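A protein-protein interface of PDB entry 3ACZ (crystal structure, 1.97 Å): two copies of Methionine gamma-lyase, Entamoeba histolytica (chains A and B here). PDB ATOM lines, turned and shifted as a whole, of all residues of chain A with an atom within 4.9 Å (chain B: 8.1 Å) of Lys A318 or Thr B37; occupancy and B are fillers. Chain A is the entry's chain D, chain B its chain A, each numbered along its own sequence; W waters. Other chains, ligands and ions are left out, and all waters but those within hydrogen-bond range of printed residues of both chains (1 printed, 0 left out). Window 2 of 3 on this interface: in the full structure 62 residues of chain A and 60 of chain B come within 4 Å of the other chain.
The side-chain hydroxyl of Thr B37 is in hydrogen-bond range of the side-chain carboxylate of Glu A322 (2.6 Å).
The backbone carbonyl oxygen of Leu A329 lies within hydrogen-bond range of the backbone NH of Phe B34 (2.9 Å).
OG of Ser B36 is in hydrogen-bond range of N of Gln B39 (3.1 Å).
Among the printed residues, pairs that only touch across the chains: Lys A318 with Thr B37, Met A321 with Thr B37, Glu A322 with Ser B36, Leu A329 with Ser B36, Leu A329 with Thr B37, Met A346 with Phe B34, Met A346 with Thr B37 and Met A346 with Phe B44.
Lys A318 touches one residue of chain B.
Printed residues of chain B within 4 Å of Leu A329: Phe B34 (2.9 Å), Ser B36 (3.5 Å) and Thr B37 (3.8 Å).
Of the printed residues of chain B, Met A346 touches Phe B34, Thr B37 and Phe B44.
Of the printed residues of chain A, Phe B34 touches Leu A329 and Met A346.
Printed residues of chain A within 4 Å of Ser B36: Glu A322 (3.6 Å) and Leu A329 (3.5 Å).
Thr B37 touches five residues of chain A.
Gln B38 touches none of the printed residues of chain A.
Asp B42 touches none of the printed residues of chain A.
Of the printed residues of chain A, Phe B44 touches Met A346.
The nearest residue of chain A that does not touch Thr B37 is Phe A314 (4.7 Å).
Of the 11 printed residues of chain A, 5 touch a printed residue of chain B.
Hydrophobic or aromatic side chains of chain A within 4 Å of the printed part of chain B: Met A321, Leu A329 and Met A346.
Of the 11 printed residues of chain B, 4 touch a printed residue of chain A.
Printed residues of chain B that touch a printed residue of chain A: Phe B34, Ser B36, Thr B37 and Phe B44.
Hydrophobic or aromatic side chains of chain B within 4 Å of the printed part of chain A: Phe B34 and Phe B44.
Among the printed residues, no Asp or Glu carboxylate lies within 4 Å of a Lys or Arg side-chain nitrogen of the other chain.
No position is printed for both chains.
Water W1 lies within hydrogen-bond range of OE1 of Glu A322 (2.7 Å), N of Gln B38 (3.0 Å) and OG1 of Thr B37 (3.0 Å).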
ATOM      1  N   PHE A 314     -11.001 -22.563  35.966  1.00  0.00           N
ATOM      2  CA  PHE A 314     -11.920 -22.467  34.828  1.00  0.00           C
ATOM      3  C   PHE A 314     -13.382 -22.552  35.280  1.00  0.00           C
ATOM      4  O   PHE A 314     -14.225 -21.800  34.788  1.00  0.00           O
ATOM      5  CB  PHE A 314     -11.645 -23.533  33.763  1.00  0.00           C
ATOM      6  CG  PHE A 314     -12.692 -23.572  32.678  1.00  0.00           C
ATOM      7  CD1 PHE A 314     -13.637 -24.596  32.637  1.00  0.00           C
ATOM      8  CD2 PHE A 314     -12.752 -22.569  31.711  1.00  0.00           C
ATOM      9  CE1 PHE A 314     -14.627 -24.620  31.639  1.00  0.00           C
ATOM     10  CE2 PHE A 314     -13.739 -22.592  30.698  1.00  0.00           C
ATOM     11  CZ  PHE A 314     -14.676 -23.617  30.669  1.00  0.00           C
ATOM     12  N   GLU A 315     -13.678 -23.478  36.201  1.00  0.00           N
ATOM     13  CA  GLU A 315     -15.048 -23.647  36.711  1.00  0.00           C
ATOM     14  C   GLU A 315     -15.607 -22.366  37.311  1.00  0.00           C
ATOM     15  O   GLU A 315     -16.774 -22.036  37.099  1.00  0.00           O
ATOM     16  CB  GLU A 315     -15.166 -24.798  37.717  1.00  0.00           C
ATOM     17  CG  GLU A 315     -15.168 -26.194  37.075  1.00  0.00           C
ATOM     18  CD  GLU A 315     -16.224 -26.351  35.970  1.00  0.00           C
ATOM     19  OE1 GLU A 315     -15.874 -26.823  34.854  1.00  0.00           O
ATOM     20  OE2 GLU A 315     -17.402 -25.980  36.207  1.00  0.00           O
ATOM     21  N   ALA A 316     -14.763 -21.648  38.048  1.00  0.00           N
ATOM     22  CA  ALA A 316     -15.132 -20.354  38.602  1.00  0.00           C
ATOM     23  C   ALA A 316     -15.394 -19.309  37.509  1.00  0.00           C
ATOM     24  O   ALA A 316     -16.312 -18.488  37.630  1.00  0.00           O
ATOM     25  CB  ALA A 316     -14.064 -19.871  39.588  1.00  0.00           C
ATOM     26  N   ALA A 317     -14.590 -19.329  36.445  1.00  0.00           N
ATOM     27  CA  ALA A 317     -14.798 -18.402  35.340  1.00  0.00           C
ATOM     28  C   ALA A 317     -16.116 -18.686  34.627  1.00  0.00           C
ATOM     29  O   ALA A 317     -16.893 -17.774  34.329  1.00  0.00           O
ATOM     30  CB  ALA A 317     -13.632 -18.455  34.378  1.00  0.00           C
ATOM     31  N   LYS A 318     -16.359 -19.963  34.346  1.00  0.00           N
ATOM     32  CA  LYS A 318     -17.573 -20.404  33.670  1.00  0.00           C
ATOM     33  C   LYS A 318     -18.800 -20.002  34.489  1.00  0.00           C
ATOM     34  O   LYS A 318     -19.786 -19.509  33.952  1.00  0.00           O
ATOM     35  CB  LYS A 318     -17.524 -21.918  33.463  1.00  0.00           C
ATOM     36  CG  LYS A 318     -18.794 -22.528  32.901  1.00  0.00           C
ATOM     37  CD  LYS A 318     -18.746 -24.049  32.956  1.00  0.00           C
ATOM     38  CE  LYS A 318     -20.107 -24.638  32.641  1.00  0.00           C
ATOM     39  NZ  LYS A 318     -20.014 -26.105  32.461  1.00  0.00           N
ATOM     40  N   LYS A 319     -18.729 -20.221  35.796  1.00  0.00           N
ATOM     41  CA  LYS A 319     -19.802 -19.821  36.700  1.00  0.00           C
ATOM     42  C   LYS A 319     -20.086 -18.305  36.641  1.00  0.00           C
ATOM     43  O   LYS A 319     -21.251 -17.895  36.509  1.00  0.00           O
ATOM     44  CB  LYS A 319     -19.498 -20.283  38.134  1.00  0.00           C
ATOM     45  CG  LYS A 319     -20.733 -20.638  38.950  1.00  0.00           C
ATOM     46  CD  LYS A 319     -20.367 -21.231  40.305  1.00  0.00           C
ATOM     47  CE  LYS A 319     -21.584 -21.296  41.239  1.00  0.00           C
ATOM     48  NZ  LYS A 319     -21.152 -21.604  42.615  1.00  0.00           N
ATOM     49  N   LEU A 320     -19.036 -17.483  36.724  1.00  0.00           N
ATOM     50  CA  LEU A 320     -19.213 -16.038  36.666  1.00  0.00           C
ATOM     51  C   LEU A 320     -19.821 -15.610  35.329  1.00  0.00           C
ATOM     52  O   LEU A 320     -20.805 -14.875  35.301  1.00  0.00           O
ATOM     53  CB  LEU A 320     -17.895 -15.295  36.897  1.00  0.00           C
ATOM     54  CG  LEU A 320     -17.904 -13.797  36.507  1.00  0.00           C
ATOM     55  CD1 LEU A 320     -18.829 -12.948  37.388  1.00  0.00           C
ATOM     56  CD2 LEU A 320     -16.482 -13.257  36.535  1.00  0.00           C
ATOM     57  N   MET A 321     -19.241 -16.095  34.233  1.00  0.00           N
ATOM     58  CA  MET A 321     -19.647 -15.683  32.883  1.00  0.00           C
ATOM     59  C   MET A 321     -21.056 -16.111  32.520  1.00  0.00           C
ATOM     60  O   MET A 321     -21.701 -15.482  31.683  1.00  0.00           O
ATOM     61  CB  MET A 321     -18.666 -16.210  31.839  1.00  0.00           C
ATOM     62  CG  MET A 321     -17.351 -15.451  31.790  1.00  0.00           C
ATOM     63  SD  MET A 321     -16.339 -16.074  30.428  1.00  0.00           S
ATOM     64  CE  MET A 321     -15.992 -17.732  31.022  1.00  0.00           C
ATOM     65  N   GLU A 322     -21.540 -17.171  33.155  1.00  0.00           N
ATOM     66  CA  GLU A 322     -22.848 -17.717  32.789  1.00  0.00           C
ATOM     67  C   GLU A 322     -23.990 -17.321  33.735  1.00  0.00           C
ATOM     68  O   GLU A 322     -25.125 -17.751  33.529  1.00  0.00           O
ATOM     69  CB  GLU A 322     -22.777 -19.242  32.650  1.00  0.00           C
ATOM     70  CG  GLU A 322     -22.015 -19.701  31.433  1.00  0.00           C
ATOM     71  CD  GLU A 322     -21.842 -21.209  31.373  1.00  0.00           C
ATOM     72  OE1 GLU A 322     -21.220 -21.687  30.410  1.00  0.00           O
ATOM     73  OE2 GLU A 322     -22.318 -21.919  32.279  1.00  0.00           O
ATOM     74  N   LEU A 329     -22.584 -12.064  27.390  1.00  0.00           N
ATOM     75  CA  LEU A 329     -21.534 -12.961  26.922  1.00  0.00           C
ATOM     76  C   LEU A 329     -21.452 -12.883  25.393  1.00  0.00           C
ATOM     77  O   LEU A 329     -22.354 -13.350  24.707  1.00  0.00           O
ATOM     78  CB  LEU A 329     -21.864 -14.381  27.358  1.00  0.00           C
ATOM     79  CG  LEU A 329     -20.800 -15.452  27.152  1.00  0.00           C
ATOM     80  CD1 LEU A 329     -19.522 -15.171  27.955  1.00  0.00           C
ATOM     81  CD2 LEU A 329     -21.398 -16.799  27.531  1.00  0.00           C
ATOM     82  N   MET A 346     -12.317 -18.504  23.147  1.00  0.00           N
ATOM     83  CA  MET A 346     -13.043 -17.621  22.219  1.00  0.00           C
ATOM     84  C   MET A 346     -12.076 -16.755  21.390  1.00  0.00           C
ATOM     85  O   MET A 346     -11.505 -17.255  20.434  1.00  0.00           O
ATOM     86  CB  MET A 346     -14.118 -16.781  22.935  1.00  0.00           C
ATOM     87  CG  MET A 346     -15.173 -17.610  23.691  1.00  0.00           C
ATOM     88  SD  MET A 346     -16.334 -16.611  24.660  1.00  0.00           S
ATOM     89  CE  MET A 346     -17.119 -17.826  25.716  1.00  0.00           C
ATOM     90  N   PHE B  34     -23.809 -15.279  23.085  1.00  0.00           N
ATOM     91  CA  PHE B  34     -23.670 -16.699  23.297  1.00  0.00           C
ATOM     92  C   PHE B  34     -24.616 -17.138  24.410  1.00  0.00           C
ATOM     93  O   PHE B  34     -24.788 -16.429  25.426  1.00  0.00           O
ATOM     94  CB  PHE B  34     -22.217 -17.065  23.669  1.00  0.00           C
ATOM     95  CG  PHE B  34     -21.187 -16.789  22.575  1.00  0.00           C
ATOM     96  CD1 PHE B  34     -21.460 -17.067  21.230  1.00  0.00           C
ATOM     97  CD2 PHE B  34     -19.922 -16.300  22.900  1.00  0.00           C
ATOM     98  CE1 PHE B  34     -20.501 -16.832  20.244  1.00  0.00           C
ATOM     99  CE2 PHE B  34     -18.954 -16.076  21.907  1.00  0.00           C
ATOM    100  CZ  PHE B  34     -19.263 -16.352  20.564  1.00  0.00           C
ATOM    101  N   ASP B  35     -25.220 -18.313  24.251  1.00  0.00           N
ATOM    102  CA  ASP B  35     -26.020 -18.903  25.341  1.00  0.00           C
ATOM    103  C   ASP B  35     -25.197 -19.327  26.575  1.00  0.00           C
ATOM    104  O   ASP B  35     -25.728 -19.390  27.693  1.00  0.00           O
ATOM    105  CB  ASP B  35     -26.792 -20.130  24.852  1.00  0.00           C
ATOM    106  CG  ASP B  35     -27.640 -19.850  23.624  1.00  0.00           C
ATOM    107  OD1 ASP B  35     -28.290 -18.770  23.536  1.00  0.00           O
ATOM    108  OD2 ASP B  35     -27.667 -20.752  22.760  1.00  0.00           O
ATOM    109  N   SER B  36     -23.921 -19.656  26.359  1.00  0.00           N
ATOM    110  CA  SER B  36     -23.070 -20.256  27.402  1.00  0.00           C
ATOM    111  C   SER B  36     -21.633 -20.253  26.920  1.00  0.00           C
ATOM    112  O   SER B  36     -21.385 -20.042  25.731  1.00  0.00           O
ATOM    113  CB  SER B  36     -23.493 -21.699  27.669  1.00  0.00           C
ATOM    114  OG  SER B  36     -23.223 -22.521  26.541  1.00  0.00           O
ATOM    115  N   THR B  37     -20.688 -20.486  27.829  1.00  0.00           N
ATOM    116  CA  THR B  37     -19.264 -20.536  27.457  1.00  0.00           C
ATOM    117  C   THR B  37     -19.012 -21.630  26.401  1.00  0.00           C
ATOM    118  O   THR B  37     -18.320 -21.398  25.390  1.00  0.00           O
ATOM    119  CB  THR B  37     -18.353 -20.771  28.694  1.00  0.00           C
ATOM    120  OG1 THR B  37     -18.858 -21.883  29.433  1.00  0.00           O
ATOM    121  CG2 THR B  37     -18.373 -19.583  29.620  1.00  0.00           C
ATOM    122  N   GLN B  38     -19.605 -22.802  26.637  1.00  0.00           N
ATOM    123  CA  GLN B  38     -19.490 -23.969  25.750  1.00  0.00           C
ATOM    124  C   GLN B  38     -20.037 -23.726  24.336  1.00  0.00           C
ATOM    125  O   GLN B  38     -19.403 -24.093  23.336  1.00  0.00           O
ATOM    126  CB  GLN B  38     -20.179 -25.197  26.365  1.00  0.00           C
ATOM    127  CG  GLN B  38     -19.749 -26.523  25.710  1.00  0.00           C
ATOM    128  CD  GLN B  38     -18.227 -26.700  25.700  1.00  0.00           C
ATOM    129  OE1 GLN B  38     -17.594 -26.800  26.748  1.00  0.00           O
ATOM    130  NE2 GLN B  38     -17.639 -26.714  24.508  1.00  0.00           N
ATOM    131  N   GLN B  39     -21.215 -23.118  24.259  1.00  0.00           N
ATOM    132  CA  GLN B  39     -21.831 -22.820  22.978  1.00  0.00           C
ATOM    133  C   GLN B  39     -20.930 -21.887  22.156  1.00  0.00           C
ATOM    134  O   GLN B  39     -20.746 -22.107  20.962  1.00  0.00           O
ATOM    135  CB  GLN B  39     -23.228 -22.231  23.180  1.00  0.00           C
ATOM    136  CG  GLN B  39     -24.034 -22.062  21.879  1.00  0.00           C
ATOM    137  CD  GLN B  39     -24.156 -20.616  21.428  1.00  0.00           C
ATOM    138  OE1 GLN B  39     -23.862 -19.686  22.188  1.00  0.00           O
ATOM    139  NE2 GLN B  39     -24.624 -20.414  20.184  1.00  0.00           N
ATOM    140  N   GLY B  40     -20.346 -20.881  22.816  1.00  0.00           N
ATOM    141  CA  GLY B  40     -19.377 -19.974  22.194  1.00  0.00           C
ATOM    142  C   GLY B  40     -18.084 -20.641  21.762  1.00  0.00           C
ATOM    143  O   GLY B  40     -17.596 -20.408  20.650  1.00  0.00           O
ATOM    144  N   ALA B  41     -17.517 -21.458  22.648  1.00  0.00           N
ATOM    145  CA  ALA B  41     -16.309 -22.218  22.343  1.00  0.00           C
ATOM    146  C   ALA B  41     -16.523 -23.141  21.150  1.00  0.00           C
ATOM    147  O   ALA B  41     -15.659 -23.230  20.270  1.00  0.00           O
ATOM    148  CB  ALA B  41     -15.832 -23.031  23.578  1.00  0.00           C
ATOM    149  N   ASP B  42     -17.674 -23.820  21.125  1.00  0.00           N
ATOM    150  CA  ASP B  42     -18.032 -24.705  20.026  1.00  0.00           C
ATOM    151  C   ASP B  42     -18.098 -23.959  18.685  1.00  0.00           C
ATOM    152  O   ASP B  42     -17.506 -24.421  17.701  1.00  0.00           O
ATOM    153  CB  ASP B  42     -19.338 -25.460  20.313  1.00  0.00           C
ATOM    154  CG  ASP B  42     -19.168 -26.552  21.365  1.00  0.00           C
ATOM    155  OD1 ASP B  42     -18.032 -26.845  21.790  1.00  0.00           O
ATOM    156  OD2 ASP B  42     -20.182 -27.126  21.782  1.00  0.00           O
ATOM    157  N   LEU B  43     -18.768 -22.803  18.652  1.00  0.00           N
ATOM    158  CA  LEU B  43     -18.860 -22.007  17.410  1.00  0.00           C
ATOM    159  C   LEU B  43     -17.468 -21.607  16.937  1.00  0.00           C
ATOM    160  O   LEU B  43     -17.179 -21.682  15.749  1.00  0.00           O
ATOM    161  CB  LEU B  43     -19.766 -20.774  17.564  1.00  0.00           C
ATOM    162  CG  LEU B  43     -21.275 -21.007  17.629  1.00  0.00           C
ATOM    163  CD1 LEU B  43     -22.024 -19.686  17.798  1.00  0.00           C
ATOM    164  CD2 LEU B  43     -21.782 -21.752  16.369  1.00  0.00           C
ATOM    165  N   PHE B  44     -16.593 -21.214  17.869  1.00  0.00           N
ATOM    166  CA  PHE B  44     -15.187 -20.951  17.517  1.00  0.00           C
ATOM    167  C   PHE B  44     -14.420 -22.163  16.935  1.00  0.00           C
ATOM    168  O   PHE B  44     -13.493 -21.966  16.144  1.00  0.00           O
ATOM    169  CB  PHE B  44     -14.425 -20.305  18.670  1.00  0.00           C
ATOM    170  CG  PHE B  44     -14.546 -18.811  18.699  1.00  0.00           C
ATOM    171  CD1 PHE B  44     -15.440 -18.196  19.552  1.00  0.00           C
ATOM    172  CD2 PHE B  44     -13.782 -18.024  17.837  1.00  0.00           C
ATOM    173  CE1 PHE B  44     -15.562 -16.800  19.566  1.00  0.00           C
ATOM    174  CE2 PHE B  44     -13.881 -16.638  17.846  1.00  0.00           C
ATOM    175  CZ  PHE B  44     -14.773 -16.020  18.704  1.00  0.00           C
HETATM  176  O   HOH W   1     -20.962 -23.975  29.024  1.00  0.00           O
